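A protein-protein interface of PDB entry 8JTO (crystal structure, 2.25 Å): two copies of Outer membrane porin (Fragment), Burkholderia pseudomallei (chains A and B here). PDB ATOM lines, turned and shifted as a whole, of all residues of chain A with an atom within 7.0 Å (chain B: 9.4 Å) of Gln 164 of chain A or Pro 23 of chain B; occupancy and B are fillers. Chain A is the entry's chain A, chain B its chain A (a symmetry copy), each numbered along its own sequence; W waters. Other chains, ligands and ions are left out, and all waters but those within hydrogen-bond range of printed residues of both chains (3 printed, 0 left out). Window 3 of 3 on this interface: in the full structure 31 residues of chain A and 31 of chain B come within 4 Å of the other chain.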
ATOM      1  N   SER A 160     -29.960 -12.728  27.027  1.00  0.00           N
ATOM      2  CA  SER A 160     -28.619 -13.091  26.589  1.00  0.00           C
ATOM      3  C   SER A 160     -27.578 -12.055  26.979  1.00  0.00           C
ATOM      4  O   SER A 160     -26.380 -12.366  26.961  1.00  0.00           O
ATOM      5  CB  SER A 160     -28.591 -13.262  25.073  1.00  0.00           C
ATOM      6  OG  SER A 160     -28.694 -11.993  24.443  1.00  0.00           O
ATOM      7  N   ASN A 161     -28.011 -10.832  27.302  1.00  0.00           N
ATOM      8  CA  ASN A 161     -27.122  -9.731  27.677  1.00  0.00           C
ATOM      9  C   ASN A 161     -26.062  -9.463  26.609  1.00  0.00           C
ATOM     10  O   ASN A 161     -24.967  -8.997  26.920  1.00  0.00           O
ATOM     11  CB  ASN A 161     -26.448  -9.984  29.033  1.00  0.00           C
ATOM     12  CG  ASN A 161     -27.332  -9.617  30.212  1.00  0.00           C
ATOM     13  OD1 ASN A 161     -28.562  -9.634  30.116  1.00  0.00           O
ATOM     14  ND2 ASN A 161     -26.709  -9.305  31.341  1.00  0.00           N
ATOM     15  N   ASN A 162     -26.358  -9.765  25.346  1.00  0.00           N
ATOM     16  CA  ASN A 162     -25.442  -9.424  24.262  1.00  0.00           C
ATOM     17  C   ASN A 162     -26.245  -9.091  23.011  1.00  0.00           C
ATOM     18  O   ASN A 162     -27.450  -9.352  22.926  1.00  0.00           O
ATOM     19  CB  ASN A 162     -24.414 -10.534  24.007  1.00  0.00           C
ATOM     20  CG  ASN A 162     -24.992 -11.716  23.266  1.00  0.00           C
ATOM     21  OD1 ASN A 162     -24.957 -11.769  22.035  1.00  0.00           O
ATOM     22  ND2 ASN A 162     -25.456 -12.712  24.014  1.00  0.00           N
ATOM     23  N   SER A 163     -25.563  -8.478  22.037  1.00  0.00           N
ATOM     24  CA  SER A 163     -26.263  -7.911  20.885  1.00  0.00           C
ATOM     25  C   SER A 163     -26.958  -8.968  20.032  1.00  0.00           C
ATOM     26  O   SER A 163     -27.827  -8.616  19.228  1.00  0.00           O
ATOM     27  CB  SER A 163     -25.291  -7.097  20.028  1.00  0.00           C
ATOM     28  OG  SER A 163     -24.106  -7.828  19.762  1.00  0.00           O
ATOM     29  N   GLN A 164     -26.603 -10.241  20.184  1.00  0.00           N
ATOM     30  CA  GLN A 164     -27.354 -11.344  19.581  1.00  0.00           C
ATOM     31  C   GLN A 164     -28.410 -11.786  20.588  1.00  0.00           C
ATOM     32  O   GLN A 164     -28.102 -12.437  21.593  1.00  0.00           O
ATOM     33  CB  GLN A 164     -26.413 -12.472  19.184  1.00  0.00           C
ATOM     34  CG  GLN A 164     -25.408 -12.044  18.117  1.00  0.00           C
ATOM     35  CD  GLN A 164     -24.685 -13.212  17.478  1.00  0.00           C
ATOM     36  OE1 GLN A 164     -23.721 -13.729  18.041  1.00  0.00           O
ATOM     37  NE2 GLN A 164     -25.139 -13.629  16.301  1.00  0.00           N
ATOM     38  N   PHE A 165     -29.661 -11.412  20.318  1.00  0.00           N
ATOM     39  CA  PHE A 165     -30.734 -11.570  21.290  1.00  0.00           C
ATOM     40  C   PHE A 165     -31.022 -13.036  21.612  1.00  0.00           C
ATOM     41  O   PHE A 165     -31.404 -13.354  22.742  1.00  0.00           O
ATOM     42  CB  PHE A 165     -31.992 -10.872  20.767  1.00  0.00           C
ATOM     43  CG  PHE A 165     -33.102 -10.759  21.784  1.00  0.00           C
ATOM     44  CD1 PHE A 165     -33.077  -9.773  22.762  1.00  0.00           C
ATOM     45  CD2 PHE A 165     -34.177 -11.624  21.740  1.00  0.00           C
ATOM     46  CE1 PHE A 165     -34.094  -9.665  23.688  1.00  0.00           C
ATOM     47  CE2 PHE A 165     -35.204 -11.525  22.667  1.00  0.00           C
ATOM     48  CZ  PHE A 165     -35.161 -10.546  23.645  1.00  0.00           C
ATOM     49  N   ALA A 166     -30.857 -13.936  20.644  1.00  0.00           N
ATOM     50  CA  ALA A 166     -31.173 -15.348  20.840  1.00  0.00           C
ATOM     51  C   ALA A 166     -29.963 -16.181  21.231  1.00  0.00           C
ATOM     52  O   ALA A 166     -30.099 -17.390  21.433  1.00  0.00           O
ATOM     53  CB  ALA A 166     -31.803 -15.933  19.571  1.00  0.00           C
ATOM     54  N   ASN A 167     -28.791 -15.569  21.358  1.00  0.00           N
ATOM     55  CA  ASN A 167     -27.550 -16.305  21.594  1.00  0.00           C
ATOM     56  C   ASN A 167     -27.297 -16.453  23.096  1.00  0.00           C
ATOM     57  O   ASN A 167     -26.665 -15.603  23.728  1.00  0.00           O
ATOM     58  CB  ASN A 167     -26.399 -15.598  20.897  1.00  0.00           C
ATOM     59  CG  ASN A 167     -25.109 -16.366  20.993  1.00  0.00           C
ATOM     60  OD1 ASN A 167     -25.116 -17.589  21.110  1.00  0.00           O
ATOM     61  ND2 ASN A 167     -23.991 -15.652  20.969  1.00  0.00           N
ATOM     62  N   ASN A 168     -27.759 -17.584  23.649  1.00  0.00           N
ATOM     63  CA  ASN A 168     -27.705 -17.964  25.067  1.00  0.00           C
ATOM     64  C   ASN A 168     -28.748 -17.216  25.883  1.00  0.00           C
ATOM     65  O   ASN A 168     -28.417 -16.394  26.743  1.00  0.00           O
ATOM     66  CB  ASN A 168     -26.314 -17.769  25.683  1.00  0.00           C
ATOM     67  CG  ASN A 168     -26.175 -18.474  27.032  1.00  0.00           C
ATOM     68  OD1 ASN A 168     -27.062 -19.223  27.447  1.00  0.00           O
ATOM     69  ND2 ASN A 168     -25.062 -18.238  27.717  1.00  0.00           N
ATOM     70  N   ARG A 169     -30.017 -17.508  25.618  1.00  0.00           N
ATOM     71  CA  ARG A 169     -31.130 -16.990  26.391  1.00  0.00           C
ATOM     72  C   ARG A 169     -32.041 -18.158  26.758  1.00  0.00           C
ATOM     73  O   ARG A 169     -31.855 -19.284  26.291  1.00  0.00           O
ATOM     74  CB  ARG A 169     -31.890 -15.897  25.610  1.00  0.00           C
ATOM     75  CG  ARG A 169     -32.504 -16.369  24.296  1.00  0.00           C
ATOM     76  CD  ARG A 169     -33.951 -16.845  24.474  1.00  0.00           C
ATOM     77  NE  ARG A 169     -34.533 -17.234  23.196  1.00  0.00           N
ATOM     78  CZ  ARG A 169     -35.063 -16.378  22.332  1.00  0.00           C
ATOM     79  NH1 ARG A 169     -35.145 -15.083  22.603  1.00  0.00           N
ATOM     80  NH2 ARG A 169     -35.508 -16.829  21.161  1.00  0.00           N
ATOM     81  N   ASN A 193     -29.052 -21.830  22.487  1.00  0.00           N
ATOM     82  CA  ASN A 193     -27.597 -21.677  22.529  1.00  0.00           C
ATOM     83  C   ASN A 193     -27.082 -21.638  23.965  1.00  0.00           C
ATOM     84  O   ASN A 193     -26.241 -20.808  24.319  1.00  0.00           O
ATOM     85  CB  ASN A 193     -27.148 -20.434  21.757  1.00  0.00           C
ATOM     86  CG  ASN A 193     -27.026 -20.689  20.269  1.00  0.00           C
ATOM     87  OD1 ASN A 193     -27.679 -21.582  19.720  1.00  0.00           O
ATOM     88  ND2 ASN A 193     -26.199 -19.894  19.603  1.00  0.00           N
ATOM     89  N   ASN A 197     -21.794 -18.552  25.754  1.00  0.00           N
ATOM     90  CA  ASN A 197     -20.983 -17.391  26.098  1.00  0.00           C
ATOM     91  C   ASN A 197     -21.071 -17.167  27.603  1.00  0.00           C
ATOM     92  O   ASN A 197     -21.748 -17.903  28.326  1.00  0.00           O
ATOM     93  CB  ASN A 197     -21.433 -16.151  25.318  1.00  0.00           C
ATOM     94  CG  ASN A 197     -22.945 -15.927  25.394  1.00  0.00           C
ATOM     95  OD1 ASN A 197     -23.541 -15.986  26.477  1.00  0.00           O
ATOM     96  ND2 ASN A 197     -23.567 -15.672  24.247  1.00  0.00           N
ATOM     97  N   VAL B  20     -25.408  -1.939  19.361  1.00  0.00           N
ATOM     98  CA  VAL B  20     -24.179  -2.593  19.778  1.00  0.00           C
ATOM     99  C   VAL B  20     -23.770  -3.532  18.655  1.00  0.00           C
ATOM    100  O   VAL B  20     -24.597  -4.307  18.163  1.00  0.00           O
ATOM    101  CB  VAL B  20     -24.355  -3.356  21.105  1.00  0.00           C
ATOM    102  CG1 VAL B  20     -23.128  -4.212  21.392  1.00  0.00           C
ATOM    103  CG2 VAL B  20     -24.611  -2.375  22.261  1.00  0.00           C
ATOM    104  N   ALA B  21     -22.511  -3.440  18.233  1.00  0.00           N
ATOM    105  CA  ALA B  21     -22.030  -4.258  17.128  1.00  0.00           C
ATOM    106  C   ALA B  21     -22.197  -5.741  17.433  1.00  0.00           C
ATOM    107  O   ALA B  21     -21.957  -6.197  18.557  1.00  0.00           O
ATOM    108  CB  ALA B  21     -20.555  -3.951  16.837  1.00  0.00           C
ATOM    109  N   THR B  22     -22.630  -6.490  16.434  1.00  0.00           N
ATOM    110  CA  THR B  22     -22.607  -7.942  16.453  1.00  0.00           C
ATOM    111  C   THR B  22     -21.402  -8.443  15.681  1.00  0.00           C
ATOM    112  O   THR B  22     -20.761  -7.685  14.950  1.00  0.00           O
ATOM    113  CB  THR B  22     -23.892  -8.494  15.842  1.00  0.00           C
ATOM    114  OG1 THR B  22     -23.929  -8.169  14.445  1.00  0.00           O
ATOM    115  CG2 THR B  22     -25.089  -7.909  16.545  1.00  0.00           C
ATOM    116  N   PRO B  23     -21.047  -9.726  15.832  1.00  0.00           N
ATOM    117  CA  PRO B  23     -19.929 -10.269  15.037  1.00  0.00           C
ATOM    118  C   PRO B  23     -20.111 -10.118  13.529  1.00  0.00           C
ATOM    119  O   PRO B  23     -19.118  -9.972  12.807  1.00  0.00           O
ATOM    120  CB  PRO B  23     -19.878 -11.748  15.459  1.00  0.00           C
ATOM    121  CG  PRO B  23     -21.083 -11.981  16.343  1.00  0.00           C
ATOM    122  CD  PRO B  23     -21.464 -10.655  16.899  1.00  0.00           C
ATOM    123  N   SER B  24     -21.347 -10.139  13.028  1.00  0.00           N
ATOM    124  CA  SER B  24     -21.573  -9.901  11.606  1.00  0.00           C
ATOM    125  C   SER B  24     -21.297  -8.464  11.193  1.00  0.00           C
ATOM    126  O   SER B  24     -21.420  -8.158  10.005  1.00  0.00           O
ATOM    127  CB  SER B  24     -23.011 -10.264  11.226  1.00  0.00           C
ATOM    128  OG  SER B  24     -23.928  -9.261  11.636  1.00  0.00           O
ATOM    129  N   GLY B  25     -20.951  -7.575  12.130  1.00  0.00           N
ATOM    130  CA  GLY B  25     -20.627  -6.200  11.818  1.00  0.00           C
ATOM    131  C   GLY B  25     -21.807  -5.252  11.791  1.00  0.00           C
ATOM    132  O   GLY B  25     -21.607  -4.035  11.808  1.00  0.00           O
ATOM    133  N   SER B  26     -23.029  -5.765  11.736  1.00  0.00           N
ATOM    134  CA  SER B  26     -24.185  -4.893  11.796  1.00  0.00           C
ATOM    135  C   SER B  26     -24.532  -4.580  13.250  1.00  0.00           C
ATOM    136  O   SER B  26     -24.176  -5.316  14.177  1.00  0.00           O
ATOM    137  CB  SER B  26     -25.373  -5.529  11.075  1.00  0.00           C
ATOM    138  OG  SER B  26     -25.975  -6.534  11.869  1.00  0.00           O
ATOM    139  N   GLY B  27     -25.210  -3.452  13.444  1.00  0.00           N
ATOM    140  CA  GLY B  27     -25.559  -2.981  14.769  1.00  0.00           C
ATOM    141  C   GLY B  27     -26.960  -3.428  15.134  1.00  0.00           C
ATOM    142  O   GLY B  27     -27.896  -3.287  14.344  1.00  0.00           O
ATOM    143  N   LYS B  28     -27.088  -3.993  16.329  1.00  0.00           N
ATOM    144  CA  LYS B  28     -28.383  -4.390  16.856  1.00  0.00           C
ATOM    145  C   LYS B  28     -28.516  -3.892  18.286  1.00  0.00           C
ATOM    146  O   LYS B  28     -27.539  -3.488  18.920  1.00  0.00           O
ATOM    147  CB  LYS B  28     -28.603  -5.917  16.784  1.00  0.00           C
ATOM    148  CG  LYS B  28     -28.523  -6.482  15.360  1.00  0.00           C
ATOM    149  CD  LYS B  28     -28.241  -7.976  15.347  1.00  0.00           C
ATOM    150  CE  LYS B  28     -27.691  -8.429  13.991  1.00  0.00           C
ATOM    151  NZ  LYS B  28     -27.011  -9.757  14.079  1.00  0.00           N
ATOM    152  N   SER B  29     -29.743  -3.904  18.787  1.00  0.00           N
ATOM    153  CA  SER B  29     -29.954  -3.465  20.153  1.00  0.00           C
ATOM    154  C   SER B  29     -29.465  -4.536  21.126  1.00  0.00           C
ATOM    155  O   SER B  29     -29.490  -5.735  20.839  1.00  0.00           O
ATOM    156  CB  SER B  29     -31.430  -3.148  20.396  1.00  0.00           C
ATOM    157  OG  SER B  29     -32.259  -4.185  19.913  1.00  0.00           O
ATOM    158  N   LEU B  30     -28.968  -4.089  22.269  1.00  0.00           N
ATOM    159  CA  LEU B  30     -28.581  -4.972  23.359  1.00  0.00           C
ATOM    160  C   LEU B  30     -29.603  -4.814  24.472  1.00  0.00           C
ATOM    161  O   LEU B  30     -29.760  -3.717  25.016  1.00  0.00           O
ATOM    162  CB  LEU B  30     -27.177  -4.634  23.864  1.00  0.00           C
ATOM    163  CG  LEU B  30     -26.477  -5.626  24.805  1.00  0.00           C
ATOM    164  CD1 LEU B  30     -24.984  -5.360  24.809  1.00  0.00           C
ATOM    165  CD2 LEU B  30     -27.003  -5.539  26.222  1.00  0.00           C
ATOM    166  N   TRP B  31     -30.287  -5.900  24.813  1.00  0.00           N
ATOM    167  CA  TRP B  31     -31.137  -5.956  25.997  1.00  0.00           C
ATOM    168  C   TRP B  31     -30.420  -6.739  27.090  1.00  0.00           C
ATOM    169  O   TRP B  31     -29.786  -7.765  26.821  1.00  0.00           O
ATOM    170  CB  TRP B  31     -32.484  -6.603  25.673  1.00  0.00           C
ATOM    171  CG  TRP B  31     -33.352  -5.743  24.801  1.00  0.00           C
ATOM    172  CD1 TRP B  31     -33.338  -5.680  23.429  1.00  0.00           C
ATOM    173  CD2 TRP B  31     -34.374  -4.839  25.234  1.00  0.00           C
ATOM    174  NE1 TRP B  31     -34.281  -4.778  22.990  1.00  0.00           N
ATOM    175  CE2 TRP B  31     -34.934  -4.254  24.076  1.00  0.00           C
ATOM    176  CE3 TRP B  31     -34.862  -4.456  26.488  1.00  0.00           C
ATOM    177  CZ2 TRP B  31     -35.957  -3.311  24.136  1.00  0.00           C
ATOM    178  CZ3 TRP B  31     -35.882  -3.521  26.543  1.00  0.00           C
ATOM    179  CH2 TRP B  31     -36.421  -2.964  25.373  1.00  0.00           C
ATOM    180  N   PRO B 336     -18.946  -4.303  22.934  1.00  0.00           N
ATOM    181  CA  PRO B 336     -18.570  -3.668  21.666  1.00  0.00           C
ATOM    182  C   PRO B 336     -19.259  -2.326  21.492  1.00  0.00           C
ATOM    183  O   PRO B 336     -20.344  -2.078  22.027  1.00  0.00           O
ATOM    184  CB  PRO B 336     -19.027  -4.669  20.593  1.00  0.00           C
ATOM    185  CG  PRO B 336     -19.633  -5.820  21.309  1.00  0.00           C
ATOM    186  CD  PRO B 336     -19.748  -5.517  22.755  1.00  0.00           C
ATOM    187  N   PHE B 337     -18.603  -1.456  20.727  1.00  0.00           N
ATOM    188  CA  PHE B 337     -19.133  -0.131  20.457  1.00  0.00           C
ATOM    189  C   PHE B 337     -20.341  -0.220  19.532  1.00  0.00           C
ATOM    190  O   PHE B 337     -20.626  -1.258  18.922  1.00  0.00           O
ATOM    191  CB  PHE B 337     -18.066   0.765  19.828  1.00  0.00           C
ATOM    192  CG  PHE B 337     -16.826   0.936  20.670  1.00  0.00           C
ATOM    193  CD1 PHE B 337     -16.860   0.728  22.042  1.00  0.00           C
ATOM    194  CD2 PHE B 337     -15.626   1.331  20.085  1.00  0.00           C
ATOM    195  CE1 PHE B 337     -15.722   0.898  22.827  1.00  0.00           C
ATOM    196  CE2 PHE B 337     -14.475   1.499  20.858  1.00  0.00           C
ATOM    197  CZ  PHE B 337     -14.523   1.286  22.233  1.00  0.00           C
ATOM    198  N   THR B 339     -22.070   0.648  16.005  1.00  0.00           N
ATOM    199  CA  THR B 339     -21.539   0.722  14.646  1.00  0.00           C
ATOM    200  C   THR B 339     -21.674   2.111  14.043  1.00  0.00           C
ATOM    201  O   THR B 339     -21.117   2.365  12.972  1.00  0.00           O
ATOM    202  CB  THR B 339     -22.237  -0.293  13.728  1.00  0.00           C
ATOM    203  OG1 THR B 339     -23.609   0.089  13.537  1.00  0.00           O
ATOM    204  CG2 THR B 339     -22.157  -1.703  14.314  1.00  0.00           C
HETATM  205  O   HOH W   1     -30.572  -9.969  25.324  1.00  0.00           O
HETATM  206  O   HOH W   2     -29.986  -8.206  22.943  1.00  0.00           O
HETATM  207  O   HOH W   3     -24.564 -11.472  14.110  1.00  0.00           O
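OG of Ser 163 of chain A sits at hydrogen-bond distance from O of Ala 21 of chain B (3.0 Å).
O of Ser 160 of chain A sits at hydrogen-bond distance from ND2 of Asn 162 of chain A (3.1 Å). The side-chain hydroxyl (OG) of Ser 160 of chain A lies within hydrogen-bond range of the backbone carbonyl oxygen (O) of Gln 164 of chain A. The side-chain hydroxyl of Ser 160 of chain A is in hydrogen-bond range of the backbone carbonyl oxygen of Phe 165 of chain A (3.5 Å). The side-chain amide nitrogen (ND2) of Asn 162 of chain A lies within hydrogen-bond range of the backbone carbonyl oxygen (O) of Asn 167 of chain A, at 3.1 Å. The backbone carbonyl oxygen of Phe 337 of chain B sits at hydrogen-bond distance from the backbone NH of Ala 21 of chain B (3.0 Å). The side-chain hydroxyl (OG1) of Thr 22 of chain B lies within hydrogen-bond range of the side-chain hydroxyl (OG) of Ser 24 of chain B, 3.0 Å away.
Among the printed residues, pairs that only touch across the chains: Ser 163 of chain A with Thr 22 of chain B, Asn 161 of chain A with Trp 31 of chain B, Ser 163 of chain A with Val 20 of chain B, Gln 164 of chain A with Pro 23 of chain B, Ser 163 of chain A with Ser 29 of chain B, Ser 163 of chain A with Lys 28 of chain B, Asn 162 of chain A with Leu 30 of chain B and Phe 165 of chain A with Trp 31 of chain B.
Of the printed residues of chain B, Gln 164 of chain A touches Pro 23. Pro 23 of chain B touches just one residue of chain A: Gln 164 (3.6 Å). Of chain B, only Leu 30 (3.9 Å) comes within 4 Å of Asn 162 of chain A. Ser 163 of chain A touches just these residues of chain B: Val 20 (3.4 Å), Ala 21 (3.0 Å), Thr 22 (3.4 Å), Lys 28 (3.7 Å) and Ser 29 (3.7 Å). No residue of chain B comes within 4 Å of Asn 167 of chain A. Of the printed residues of chain A, Ala 21 of chain B touches Ser 163 (3.0 Å). Printed residues of chain A within 4 Å of Val 20 of chain B: Ser 163. Printed residues of chain A within 4 Å of Lys 28 of chain B: Ser 163 (3.7 Å). Of the printed residues of chain A, Trp 31 of chain B touches Asn 161 and Phe 165. Printed residues of chain B within 4 Å of Phe 165 of chain A: Trp 31. Thr 339 of chain B touches none of the printed residues of chain A. Ser 24 of chain B touches none of the printed residues of chain A. The nearest residue of chain B that does not touch Gln 164 of chain A is Thr 22 of chain B (4.4 Å). The nearest residue of chain A that does not touch Pro 23 of chain B is Ser 163 of chain A (4.8 Å).
Of the 15 printed residues of chain B, 8 touch a printed residue of chain A. Among the printed residues, no Asp or Glu carboxylate lies within 4 Å of a Lys or Arg side-chain nitrogen of the other chain.
No position is printed for both chains. Of the 9 pairs that touch across the chains among the printed residues, none has its exchanged pair printed and touching as well.
Water W1 lies within hydrogen-bond range of O of Trp 31 of chain B, OG of Ser 160 of chain A and N of Asn 161 of chain A. Water W2 lies within hydrogen-bond range of O of Asn 162 of chain A, N of Trp 31 of chain B and O of Ser 29 of chain B. Water W3 lies within hydrogen-bond range of the side-chain amino group (NZ) of Lys 28 of chain B (3.0 Å), the side-chain amide nitrogen (NE2) of Gln 164 of chain A (3.1 Å), the side-chain hydroxyl (OG) of Ser 24 of chain B (3.4 Å) and the side-chain hydroxyl (OG1) of Thr 22 of chain B (3.4 Å).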
